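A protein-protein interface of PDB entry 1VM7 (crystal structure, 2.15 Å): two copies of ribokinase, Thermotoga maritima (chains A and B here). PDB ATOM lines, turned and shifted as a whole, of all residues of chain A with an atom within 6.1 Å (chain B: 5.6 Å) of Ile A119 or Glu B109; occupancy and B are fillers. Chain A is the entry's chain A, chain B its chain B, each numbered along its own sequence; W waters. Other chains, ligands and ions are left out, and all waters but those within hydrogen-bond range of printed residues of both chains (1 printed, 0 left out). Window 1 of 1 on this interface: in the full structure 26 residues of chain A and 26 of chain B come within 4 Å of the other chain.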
ATOM      1  N   ARG A 105     -24.489 -20.020  -1.739  1.00  0.00           N
ATOM      2  CA  ARG A 105     -24.661 -21.462  -1.614  1.00  0.00           C
ATOM      3  C   ARG A 105     -23.345 -22.183  -1.385  1.00  0.00           C
ATOM      4  O   ARG A 105     -22.277 -21.676  -1.729  1.00  0.00           O
ATOM      5  CB  ARG A 105     -25.435 -22.015  -2.791  1.00  0.00           C
ATOM      6  CG  ARG A 105     -24.854 -21.910  -4.162  1.00  0.00           C
ATOM      7  CD  ARG A 105     -25.980 -22.063  -5.159  1.00  0.00           C
ATOM      8  NE  ARG A 105     -26.916 -20.970  -4.981  1.00  0.00           N
ATOM      9  CZ  ARG A 105     -28.107 -20.833  -5.560  1.00  0.00           C
ATOM     10  NH1 ARG A 105     -28.585 -21.718  -6.424  1.00  0.00           N
ATOM     11  NH2 ARG A 105     -28.830 -19.767  -5.265  1.00  0.00           N
ATOM     12  N   ALA A 106     -23.413 -23.300  -0.711  1.00  0.00           N
ATOM     13  CA  ALA A 106     -22.233 -24.128  -0.490  1.00  0.00           C
ATOM     14  C   ALA A 106     -22.616 -25.527  -0.953  1.00  0.00           C
ATOM     15  O   ALA A 106     -23.706 -26.044  -0.636  1.00  0.00           O
ATOM     16  CB  ALA A 106     -21.819 -24.116   0.943  1.00  0.00           C
ATOM     17  N   PHE A 107     -21.739 -26.113  -1.753  1.00  0.00           N
ATOM     18  CA  PHE A 107     -21.955 -27.451  -2.306  1.00  0.00           C
ATOM     19  C   PHE A 107     -21.048 -28.413  -1.567  1.00  0.00           C
ATOM     20  O   PHE A 107     -19.817 -28.367  -1.726  1.00  0.00           O
ATOM     21  CB  PHE A 107     -21.619 -27.472  -3.775  1.00  0.00           C
ATOM     22  CG  PHE A 107     -22.439 -26.527  -4.574  1.00  0.00           C
ATOM     23  CD1 PHE A 107     -22.029 -25.210  -4.751  1.00  0.00           C
ATOM     24  CD2 PHE A 107     -23.632 -26.930  -5.132  1.00  0.00           C
ATOM     25  CE1 PHE A 107     -22.790 -24.338  -5.501  1.00  0.00           C
ATOM     26  CE2 PHE A 107     -24.385 -26.043  -5.908  1.00  0.00           C
ATOM     27  CZ  PHE A 107     -23.967 -24.761  -6.082  1.00  0.00           C
ATOM     28  N   ILE A 108     -21.669 -29.260  -0.755  1.00  0.00           N
ATOM     29  CA  ILE A 108     -20.965 -30.067   0.216  1.00  0.00           C
ATOM     30  C   ILE A 108     -21.072 -31.516  -0.231  1.00  0.00           C
ATOM     31  O   ILE A 108     -22.153 -32.100  -0.241  1.00  0.00           O
ATOM     32  CB  ILE A 108     -21.554 -29.910   1.647  1.00  0.00           C
ATOM     33  CG1 ILE A 108     -21.594 -28.440   2.080  1.00  0.00           C
ATOM     34  CG2 ILE A 108     -20.752 -30.790   2.663  1.00  0.00           C
ATOM     35  CD1 ILE A 108     -22.524 -28.141   3.240  1.00  0.00           C
ATOM     36  N   GLU A 109     -19.948 -32.094  -0.627  1.00  0.00           N
ATOM     37  CA  GLU A 109     -19.915 -33.505  -1.048  1.00  0.00           C
ATOM     38  C   GLU A 109     -19.459 -34.317   0.129  1.00  0.00           C
ATOM     39  O   GLU A 109     -18.392 -34.068   0.628  1.00  0.00           O
ATOM     40  CB  GLU A 109     -18.986 -33.680  -2.251  1.00  0.00           C
ATOM     41  CG  GLU A 109     -18.856 -35.108  -2.771  1.00  0.00           C
ATOM     42  CD  GLU A 109     -18.005 -35.227  -4.056  1.00  0.00           C
ATOM     43  OE1 GLU A 109     -17.498 -34.201  -4.583  1.00  0.00           O
ATOM     44  OE2 GLU A 109     -17.867 -36.363  -4.547  1.00  0.00           O
ATOM     45  N   ARG A 117     -16.108 -32.359   1.509  1.00  0.00           N
ATOM     46  CA  ARG A 117     -15.404 -31.189   0.956  1.00  0.00           C
ATOM     47  C   ARG A 117     -16.457 -30.268   0.390  1.00  0.00           C
ATOM     48  O   ARG A 117     -17.582 -30.705   0.151  1.00  0.00           O
ATOM     49  CB  ARG A 117     -14.408 -31.586  -0.142  1.00  0.00           C
ATOM     50  CG  ARG A 117     -15.072 -32.260  -1.325  1.00  0.00           C
ATOM     51  CD  ARG A 117     -14.073 -32.653  -2.349  1.00  0.00           C
ATOM     52  NE  ARG A 117     -14.682 -33.436  -3.407  1.00  0.00           N
ATOM     53  CZ  ARG A 117     -14.044 -34.386  -4.078  1.00  0.00           C
ATOM     54  NH1 ARG A 117     -12.776 -34.694  -3.786  1.00  0.00           N
ATOM     55  NH2 ARG A 117     -14.692 -35.085  -5.000  1.00  0.00           N
ATOM     56  N   ILE A 118     -16.086 -29.009   0.196  1.00  0.00           N
ATOM     57  CA  ILE A 118     -17.055 -27.927   0.043  1.00  0.00           C
ATOM     58  C   ILE A 118     -16.579 -26.928  -1.015  1.00  0.00           C
ATOM     59  O   ILE A 118     -15.428 -26.444  -0.974  1.00  0.00           O
ATOM     60  CB  ILE A 118     -17.248 -27.189   1.397  1.00  0.00           C
ATOM     61  CG1 ILE A 118     -17.604 -28.161   2.521  1.00  0.00           C
ATOM     62  CG2 ILE A 118     -18.293 -26.157   1.319  1.00  0.00           C
ATOM     63  CD1 ILE A 118     -18.018 -27.440   3.845  1.00  0.00           C
ATOM     64  N   ILE A 119     -17.469 -26.646  -1.970  1.00  0.00           N
ATOM     65  CA  ILE A 119     -17.319 -25.508  -2.857  1.00  0.00           C
ATOM     66  C   ILE A 119     -18.320 -24.437  -2.429  1.00  0.00           C
ATOM     67  O   ILE A 119     -19.518 -24.714  -2.349  1.00  0.00           O
ATOM     68  CB  ILE A 119     -17.590 -25.884  -4.294  1.00  0.00           C
ATOM     69  CG1 ILE A 119     -16.496 -26.841  -4.821  1.00  0.00           C
ATOM     70  CG2 ILE A 119     -17.602 -24.635  -5.151  1.00  0.00           C
ATOM     71  CD1 ILE A 119     -16.953 -27.649  -6.041  1.00  0.00           C
ATOM     72  N   ILE A 120     -17.813 -23.230  -2.178  1.00  0.00           N
ATOM     73  CA  ILE A 120     -18.601 -22.129  -1.684  1.00  0.00           C
ATOM     74  C   ILE A 120     -18.764 -21.070  -2.756  1.00  0.00           C
ATOM     75  O   ILE A 120     -17.783 -20.602  -3.293  1.00  0.00           O
ATOM     76  CB  ILE A 120     -17.947 -21.479  -0.439  1.00  0.00           C
ATOM     77  CG1 ILE A 120     -18.090 -22.434   0.739  1.00  0.00           C
ATOM     78  CG2 ILE A 120     -18.654 -20.141  -0.103  1.00  0.00           C
ATOM     79  CD1 ILE A 120     -17.389 -22.000   1.969  1.00  0.00           C
ATOM     80  N   PHE A 121     -20.016 -20.706  -3.042  1.00  0.00           N
ATOM     81  CA  PHE A 121     -20.321 -19.622  -3.957  1.00  0.00           C
ATOM     82  C   PHE A 121     -20.916 -18.508  -3.139  1.00  0.00           C
ATOM     83  O   PHE A 121     -22.068 -18.589  -2.677  1.00  0.00           O
ATOM     84  CB  PHE A 121     -21.275 -20.076  -5.031  1.00  0.00           C
ATOM     85  CG  PHE A 121     -21.696 -18.979  -5.961  1.00  0.00           C
ATOM     86  CD1 PHE A 121     -20.814 -18.456  -6.860  1.00  0.00           C
ATOM     87  CD2 PHE A 121     -22.982 -18.479  -5.920  1.00  0.00           C
ATOM     88  CE1 PHE A 121     -21.219 -17.452  -7.736  1.00  0.00           C
ATOM     89  CE2 PHE A 121     -23.393 -17.504  -6.807  1.00  0.00           C
ATOM     90  CZ  PHE A 121     -22.508 -16.997  -7.694  1.00  0.00           C
ATOM     91  N   ILE B  27     -25.046 -27.397 -13.469  1.00  0.00           N
ATOM     92  CA  ILE B  27     -24.563 -26.347 -12.593  1.00  0.00           C
ATOM     93  C   ILE B  27     -23.072 -26.417 -12.664  1.00  0.00           C
ATOM     94  O   ILE B  27     -22.488 -27.369 -12.170  1.00  0.00           O
ATOM     95  CB  ILE B  27     -25.097 -26.515 -11.162  1.00  0.00           C
ATOM     96  CG1 ILE B  27     -26.633 -26.439 -11.169  1.00  0.00           C
ATOM     97  CG2 ILE B  27     -24.563 -25.387 -10.261  1.00  0.00           C
ATOM     98  CD1 ILE B  27     -27.298 -27.010  -9.950  1.00  0.00           C
ATOM     99  N   LEU B  29     -19.553 -25.244 -11.795  1.00  0.00           N
ATOM    100  CA  LEU B  29     -18.766 -24.585 -10.778  1.00  0.00           C
ATOM    101  C   LEU B  29     -17.313 -24.506 -11.245  1.00  0.00           C
ATOM    102  O   LEU B  29     -16.643 -25.498 -11.375  1.00  0.00           O
ATOM    103  CB  LEU B  29     -18.927 -25.377  -9.480  1.00  0.00           C
ATOM    104  CG  LEU B  29     -20.367 -25.498  -8.949  1.00  0.00           C
ATOM    105  CD1 LEU B  29     -20.458 -26.587  -7.923  1.00  0.00           C
ATOM    106  CD2 LEU B  29     -20.828 -24.243  -8.331  1.00  0.00           C
ATOM    107  N   VAL B  31     -13.562 -23.697 -10.680  1.00  0.00           N
ATOM    108  CA  VAL B  31     -12.628 -23.681  -9.560  1.00  0.00           C
ATOM    109  C   VAL B  31     -11.192 -23.676 -10.087  1.00  0.00           C
ATOM    110  O   VAL B  31     -10.922 -24.046 -11.237  1.00  0.00           O
ATOM    111  CB  VAL B  31     -12.825 -24.906  -8.600  1.00  0.00           C
ATOM    112  CG1 VAL B  31     -14.174 -24.827  -7.916  1.00  0.00           C
ATOM    113  CG2 VAL B  31     -12.745 -26.212  -9.350  1.00  0.00           C
ATOM    114  N   HIS B  33      -8.667 -25.524  -8.829  1.00  0.00           N
ATOM    115  CA  HIS B  33      -8.195 -26.885  -8.829  1.00  0.00           C
ATOM    116  C   HIS B  33      -9.321 -27.753  -8.300  1.00  0.00           C
ATOM    117  O   HIS B  33     -10.249 -27.277  -7.620  1.00  0.00           O
ATOM    118  CB  HIS B  33      -6.954 -27.013  -7.936  1.00  0.00           C
ATOM    119  CG  HIS B  33      -7.179 -26.494  -6.549  1.00  0.00           C
ATOM    120  ND1 HIS B  33      -6.862 -25.203  -6.181  1.00  0.00           N
ATOM    121  CD2 HIS B  33      -7.776 -27.058  -5.472  1.00  0.00           C
ATOM    122  CE1 HIS B  33      -7.227 -25.003  -4.925  1.00  0.00           C
ATOM    123  NE2 HIS B  33      -7.772 -26.119  -4.467  1.00  0.00           N
ATOM    124  N   PHE B  34      -9.268 -29.035  -8.619  1.00  0.00           N
ATOM    125  CA  PHE B  34     -10.255 -29.927  -8.074  1.00  0.00           C
ATOM    126  C   PHE B  34     -10.196 -29.882  -6.552  1.00  0.00           C
ATOM    127  O   PHE B  34      -9.128 -29.980  -5.947  1.00  0.00           O
ATOM    128  CB  PHE B  34     -10.048 -31.338  -8.586  1.00  0.00           C
ATOM    129  CG  PHE B  34     -10.546 -31.543  -9.986  1.00  0.00           C
ATOM    130  CD1 PHE B  34     -11.890 -31.416 -10.262  1.00  0.00           C
ATOM    131  CD2 PHE B  34      -9.681 -31.872 -11.011  1.00  0.00           C
ATOM    132  CE1 PHE B  34     -12.379 -31.628 -11.531  1.00  0.00           C
ATOM    133  CE2 PHE B  34     -10.175 -32.069 -12.306  1.00  0.00           C
ATOM    134  CZ  PHE B  34     -11.513 -31.946 -12.556  1.00  0.00           C
ATOM    135  N   THR B  35     -11.357 -29.658  -5.947  1.00  0.00           N
ATOM    136  CA  THR B  35     -11.464 -29.594  -4.496  1.00  0.00           C
ATOM    137  C   THR B  35     -11.024 -30.937  -3.882  1.00  0.00           C
ATOM    138  O   THR B  35     -11.437 -32.016  -4.324  1.00  0.00           O
ATOM    139  CB  THR B  35     -12.902 -29.195  -4.072  1.00  0.00           C
ATOM    140  OG1 THR B  35     -13.342 -28.050  -4.828  1.00  0.00           O
ATOM    141  CG2 THR B  35     -12.941 -28.837  -2.587  1.00  0.00           C
ATOM    142  N   GLU B  39     -11.218 -30.074   2.021  1.00  0.00           N
ATOM    143  CA  GLU B  39     -10.938 -28.720   1.546  1.00  0.00           C
ATOM    144  C   GLU B  39     -12.246 -27.955   1.316  1.00  0.00           C
ATOM    145  O   GLU B  39     -13.245 -28.532   0.891  1.00  0.00           O
ATOM    146  CB  GLU B  39     -10.112 -28.771   0.257  1.00  0.00           C
ATOM    147  CG  GLU B  39      -9.941 -27.413  -0.443  1.00  0.00           C
ATOM    148  CD  GLU B  39      -9.099 -27.487  -1.713  1.00  0.00           C
ATOM    149  OE1 GLU B  39      -8.932 -28.605  -2.266  1.00  0.00           O
ATOM    150  OE2 GLU B  39      -8.606 -26.419  -2.141  1.00  0.00           O
ATOM    151  N   THR B  40     -12.226 -26.672   1.650  1.00  0.00           N
ATOM    152  CA  THR B  40     -13.283 -25.741   1.316  1.00  0.00           C
ATOM    153  C   THR B  40     -12.637 -24.825   0.297  1.00  0.00           C
ATOM    154  O   THR B  40     -11.562 -24.301   0.547  1.00  0.00           O
ATOM    155  CB  THR B  40     -13.752 -24.959   2.562  1.00  0.00           C
ATOM    156  OG1 THR B  40     -14.394 -25.854   3.454  1.00  0.00           O
ATOM    157  CG2 THR B  40     -14.775 -23.860   2.187  1.00  0.00           C
ATOM    158  N   GLN B  41     -13.245 -24.687  -0.874  1.00  0.00           N
ATOM    159  CA  GLN B  41     -12.683 -23.862  -1.948  1.00  0.00           C
ATOM    160  C   GLN B  41     -13.784 -22.981  -2.483  1.00  0.00           C
ATOM    161  O   GLN B  41     -14.894 -23.443  -2.620  1.00  0.00           O
ATOM    162  CB  GLN B  41     -12.119 -24.745  -3.081  1.00  0.00           C
ATOM    163  CG  GLN B  41     -11.596 -23.943  -4.269  1.00  0.00           C
ATOM    164  CD  GLN B  41     -10.913 -24.771  -5.349  1.00  0.00           C
ATOM    165  OE1 GLN B  41     -10.053 -24.259  -6.073  1.00  0.00           O
ATOM    166  NE2 GLN B  41     -11.297 -26.033  -5.477  1.00  0.00           N
ATOM    167  N   LYS B  42     -13.488 -21.713  -2.757  1.00  0.00           N
ATOM    168  CA  LYS B  42     -14.449 -20.806  -3.374  1.00  0.00           C
ATOM    169  C   LYS B  42     -14.583 -21.119  -4.857  1.00  0.00           C
ATOM    170  O   LYS B  42     -13.582 -21.339  -5.535  1.00  0.00           O
ATOM    171  CB  LYS B  42     -14.015 -19.353  -3.222  1.00  0.00           C
ATOM    172  CG  LYS B  42     -14.118 -18.822  -1.817  1.00  0.00           C
ATOM    173  CD  LYS B  42     -14.253 -17.289  -1.822  1.00  0.00           C
ATOM    174  CE  LYS B  42     -14.373 -16.695  -0.402  1.00  0.00           C
ATOM    175  NZ  LYS B  42     -14.745 -15.217  -0.464  1.00  0.00           N
ATOM    176  N   ALA B  43     -15.815 -21.121  -5.361  1.00  0.00           N
ATOM    177  CA  ALA B  43     -16.041 -21.209  -6.794  1.00  0.00           C
ATOM    178  C   ALA B  43     -15.715 -19.839  -7.404  1.00  0.00           C
ATOM    179  O   ALA B  43     -16.167 -18.808  -6.908  1.00  0.00           O
ATOM    180  CB  ALA B  43     -17.461 -21.612  -7.092  1.00  0.00           C
ATOM    181  N   PHE B 107     -24.040 -31.449 -11.036  1.00  0.00           N
ATOM    182  CA  PHE B 107     -23.093 -30.539 -10.409  1.00  0.00           C
ATOM    183  C   PHE B 107     -21.728 -30.795 -11.000  1.00  0.00           C
ATOM    184  O   PHE B 107     -21.146 -31.845 -10.785  1.00  0.00           O
ATOM    185  CB  PHE B 107     -23.050 -30.730  -8.908  1.00  0.00           C
ATOM    186  CG  PHE B 107     -24.373 -30.554  -8.240  1.00  0.00           C
ATOM    187  CD1 PHE B 107     -25.217 -31.622  -8.076  1.00  0.00           C
ATOM    188  CD2 PHE B 107     -24.776 -29.306  -7.777  1.00  0.00           C
ATOM    189  CE1 PHE B 107     -26.427 -31.478  -7.435  1.00  0.00           C
ATOM    190  CE2 PHE B 107     -26.000 -29.143  -7.137  1.00  0.00           C
ATOM    191  CZ  PHE B 107     -26.819 -30.225  -6.965  1.00  0.00           C
ATOM    192  N   ILE B 108     -21.243 -29.832 -11.764  1.00  0.00           N
ATOM    193  CA  ILE B 108     -20.096 -30.019 -12.642  1.00  0.00           C
ATOM    194  C   ILE B 108     -18.985 -29.115 -12.155  1.00  0.00           C
ATOM    195  O   ILE B 108     -19.052 -27.889 -12.327  1.00  0.00           O
ATOM    196  CB  ILE B 108     -20.431 -29.601 -14.099  1.00  0.00           C
ATOM    197  CG1 ILE B 108     -21.705 -30.301 -14.601  1.00  0.00           C
ATOM    198  CG2 ILE B 108     -19.239 -29.826 -14.999  1.00  0.00           C
ATOM    199  CD1 ILE B 108     -22.168 -29.783 -15.969  1.00  0.00           C
ATOM    200  N   GLU B 109     -17.983 -29.723 -11.536  1.00  0.00           N
ATOM    201  CA  GLU B 109     -16.843 -28.993 -11.047  1.00  0.00           C
ATOM    202  C   GLU B 109     -15.821 -28.996 -12.168  1.00  0.00           C
ATOM    203  O   GLU B 109     -15.452 -30.059 -12.652  1.00  0.00           O
ATOM    204  CB  GLU B 109     -16.293 -29.664  -9.771  1.00  0.00           C
ATOM    205  CG  GLU B 109     -15.150 -28.894  -9.141  1.00  0.00           C
ATOM    206  CD  GLU B 109     -14.615 -29.543  -7.840  1.00  0.00           C
ATOM    207  OE1 GLU B 109     -15.121 -30.601  -7.416  1.00  0.00           O
ATOM    208  OE2 GLU B 109     -13.674 -28.985  -7.273  1.00  0.00           O
ATOM    209  N   VAL B 110     -15.378 -27.806 -12.581  1.00  0.00           N
ATOM    210  CA  VAL B 110     -14.412 -27.676 -13.668  1.00  0.00           C
ATOM    211  C   VAL B 110     -13.219 -26.834 -13.210  1.00  0.00           C
ATOM    212  O   VAL B 110     -13.401 -25.690 -12.742  1.00  0.00           O
ATOM    213  CB  VAL B 110     -15.097 -27.135 -14.965  1.00  0.00           C
ATOM    214  CG1 VAL B 110     -15.898 -25.925 -14.718  1.00  0.00           C
ATOM    215  CG2 VAL B 110     -14.083 -26.879 -16.052  1.00  0.00           C
ATOM    216  N   ASP B 111     -12.003 -27.398 -13.334  1.00  0.00           N
ATOM    217  CA  ASP B 111     -10.805 -26.721 -12.897  1.00  0.00           C
ATOM    218  C   ASP B 111     -10.285 -25.792 -13.981  1.00  0.00           C
ATOM    219  O   ASP B 111     -10.894 -25.674 -15.025  1.00  0.00           O
ATOM    220  CB  ASP B 111      -9.760 -27.719 -12.388  1.00  0.00           C
ATOM    221  CG  ASP B 111      -9.066 -28.505 -13.488  1.00  0.00           C
ATOM    222  OD1 ASP B 111      -9.320 -28.306 -14.702  1.00  0.00           O
ATOM    223  OD2 ASP B 111      -8.223 -29.342 -13.094  1.00  0.00           O
ATOM    224  N   GLN B 115     -10.615 -29.613 -17.136  1.00  0.00           N
ATOM    225  CA  GLN B 115     -11.043 -30.934 -16.693  1.00  0.00           C
ATOM    226  C   GLN B 115     -12.247 -30.765 -15.782  1.00  0.00           C
ATOM    227  O   GLN B 115     -12.340 -29.804 -15.009  1.00  0.00           O
ATOM    228  CB  GLN B 115      -9.945 -31.684 -15.937  1.00  0.00           C
ATOM    229  CG  GLN B 115     -10.390 -33.072 -15.319  1.00  0.00           C
ATOM    230  CD  GLN B 115     -10.768 -34.171 -16.319  1.00  0.00           C
ATOM    231  OE1 GLN B 115     -11.860 -34.153 -16.932  1.00  0.00           O
ATOM    232  NE2 GLN B 115      -9.872 -35.160 -16.455  1.00  0.00           N
ATOM    233  N   ASN B 116     -13.152 -31.729 -15.828  1.00  0.00           N
ATOM    234  CA  ASN B 116     -14.289 -31.692 -14.949  1.00  0.00           C
ATOM    235  C   ASN B 116     -14.588 -33.039 -14.305  1.00  0.00           C
ATOM    236  O   ASN B 116     -14.033 -34.079 -14.658  1.00  0.00           O
ATOM    237  CB  ASN B 116     -15.541 -31.126 -15.680  1.00  0.00           C
ATOM    238  CG  ASN B 116     -16.197 -32.135 -16.680  1.00  0.00           C
ATOM    239  OD1 ASN B 116     -16.054 -33.345 -16.563  1.00  0.00           O
ATOM    240  ND2 ASN B 116     -16.946 -31.601 -17.643  1.00  0.00           N
ATOM    241  N   ARG B 117     -15.466 -32.977 -13.331  1.00  0.00           N
ATOM    242  CA  ARG B 117     -16.149 -34.143 -12.811  1.00  0.00           C
ATOM    243  C   ARG B 117     -17.557 -33.697 -12.468  1.00  0.00           C
ATOM    244  O   ARG B 117     -17.859 -32.477 -12.403  1.00  0.00           O
ATOM    245  CB  ARG B 117     -15.443 -34.726 -11.607  1.00  0.00           C
ATOM    246  CG  ARG B 117     -15.404 -33.832 -10.426  1.00  0.00           C
ATOM    247  CD  ARG B 117     -14.555 -34.413  -9.335  1.00  0.00           C
ATOM    248  NE  ARG B 117     -14.338 -33.376  -8.338  1.00  0.00           N
ATOM    249  CZ  ARG B 117     -13.346 -33.347  -7.467  1.00  0.00           C
ATOM    250  NH1 ARG B 117     -12.432 -34.315  -7.434  1.00  0.00           N
ATOM    251  NH2 ARG B 117     -13.277 -32.323  -6.619  1.00  0.00           N
ATOM    252  N   ILE B 118     -18.413 -34.686 -12.241  1.00  0.00           N
ATOM    253  CA  ILE B 118     -19.845 -34.476 -12.200  1.00  0.00           C
ATOM    254  C   ILE B 118     -20.543 -35.358 -11.168  1.00  0.00           C
ATOM    255  O   ILE B 118     -20.375 -36.580 -11.160  1.00  0.00           O
ATOM    256  CB  ILE B 118     -20.499 -34.764 -13.601  1.00  0.00           C
ATOM    257  CG1 ILE B 118     -19.834 -33.931 -14.710  1.00  0.00           C
ATOM    258  CG2 ILE B 118     -22.010 -34.550 -13.552  1.00  0.00           C
ATOM    259  CD1 ILE B 118     -20.499 -34.037 -16.092  1.00  0.00           C
HETATM  260  O   HOH W   1     -17.337 -33.150  -7.273  1.00  0.00           O
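N of Ile A120 lies within hydrogen-bond range of O of Gln B41, at 3.0 Å. The backbone NH (N) of Ile A118 lies within hydrogen-bond range of the backbone carbonyl oxygen (O) of Glu B39 (3.0 Å). The backbone carbonyl oxygen (O) of Ile A120 sits at hydrogen-bond distance from the backbone NH (N) of Ala B43 (2.9 Å). The guanidinium group (NH1) of Arg A117 lies within hydrogen-bond range of the backbone carbonyl oxygen (O) of Thr B35. The backbone carbonyl oxygen of Ile A118 sits at hydrogen-bond distance from the backbone NH of Gln B41 (2.8 Å). NH1 of Arg B117 sits close to NH2 of Arg A117 (3.4 Å).
O of Ile B108 sits at hydrogen-bond distance from N of Leu B29, at 2.7 Å. The side-chain carboxylate (OE2) of Glu B109 is in hydrogen-bond range of the side-chain hydroxyl (OG1) of Thr B35. The side-chain amide nitrogen of Gln B41 is in hydrogen-bond range of the side-chain hydroxyl of Thr B35 (2.9 Å). NH2 of Arg B117 is in salt-bridge range of OE1 of Glu B109, at 2.6 Å. The side-chain amide nitrogen (NE2) of Gln B41 lies within hydrogen-bond range of the backbone carbonyl oxygen (O) of His B33. O of Leu B29 sits at hydrogen-bond distance from N of Val B110 (2.9 Å).
CD2 of Leu B29 touches CE1 of Phe A107, at 3.4 Å. Phe B107 touches Phe A107 (CE2 to CE2, 3.7 Å). Glu B39 touches Arg A117 (O to CA, 3.4 Å). Thr B40 touches Ile A118. Ile A119 touches Thr B35. Ile A119 touches Gln B41. Ile A119 touches Ala B43. Glu B109 touches Ile A119. Ile A120 touches Thr B40 (CD1 to CG2, 3.2 Å). Ile A120 touches Lys B42.
Of chain B, only Thr B35, Gln B41, Ala B43 and Glu B109 come within 4 Å of Ile A119. Glu B109 touches one residue of chain A. Printed residues of chain A within 4 Å of Glu B39: Arg A117 (3.4 Å) and Ile A118 (3.0 Å). Printed residues of chain A within 4 Å of Ala B43: Ile A119 and Ile A120. Printed residues of chain B within 4 Å of Ile A118: Thr B35, Glu B39, Thr B40 and Gln B41. Printed residues of chain A within 4 Å of Thr B35: Arg A117, Ile A118 and Ile A119. The nearest residue of chain B that does not touch Ile A119 is Leu B29 (4.1 Å).
Of the 20 printed residues of chain B, 10 touch a printed residue of chain A. Hydrophobic or aromatic side chains of chain B within 4 Å of the printed part of chain A: Leu B29, Ala B43 and Phe B107. Of the 10 printed residues of chain A, 5 touch a printed residue of chain B. Printed residues of chain A that touch a printed residue of chain B: Phe A107, Arg A117, Ile A118, Ile A119 and Ile A120. Hydrophobic or aromatic side chains of chain A that line the printed part of chain B: Phe A107, Ile A118, Ile A119 and Ile A120. Among the printed residues, no Asp or Glu carboxylate lies within 4 Å of a Lys or Arg side-chain nitrogen of the other chain.
Phe B107 touches its own counterpart, Phe A107. Arg A117 touches its own counterpart, Arg B117. 5 positions are printed for both chains. Of the 17 pairs that touch across the chains among the printed residues, 2 have their exchanged pair printed and touching as well.
Water W1 lies within hydrogen-bond range of the side-chain carboxylate (OE1) of Glu A109 (2.9 Å), the guanidinium group (NE) of Arg B117 (3.2 Å) and the side-chain carboxylate (OE1) of Glu B109 (3.4 Å).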
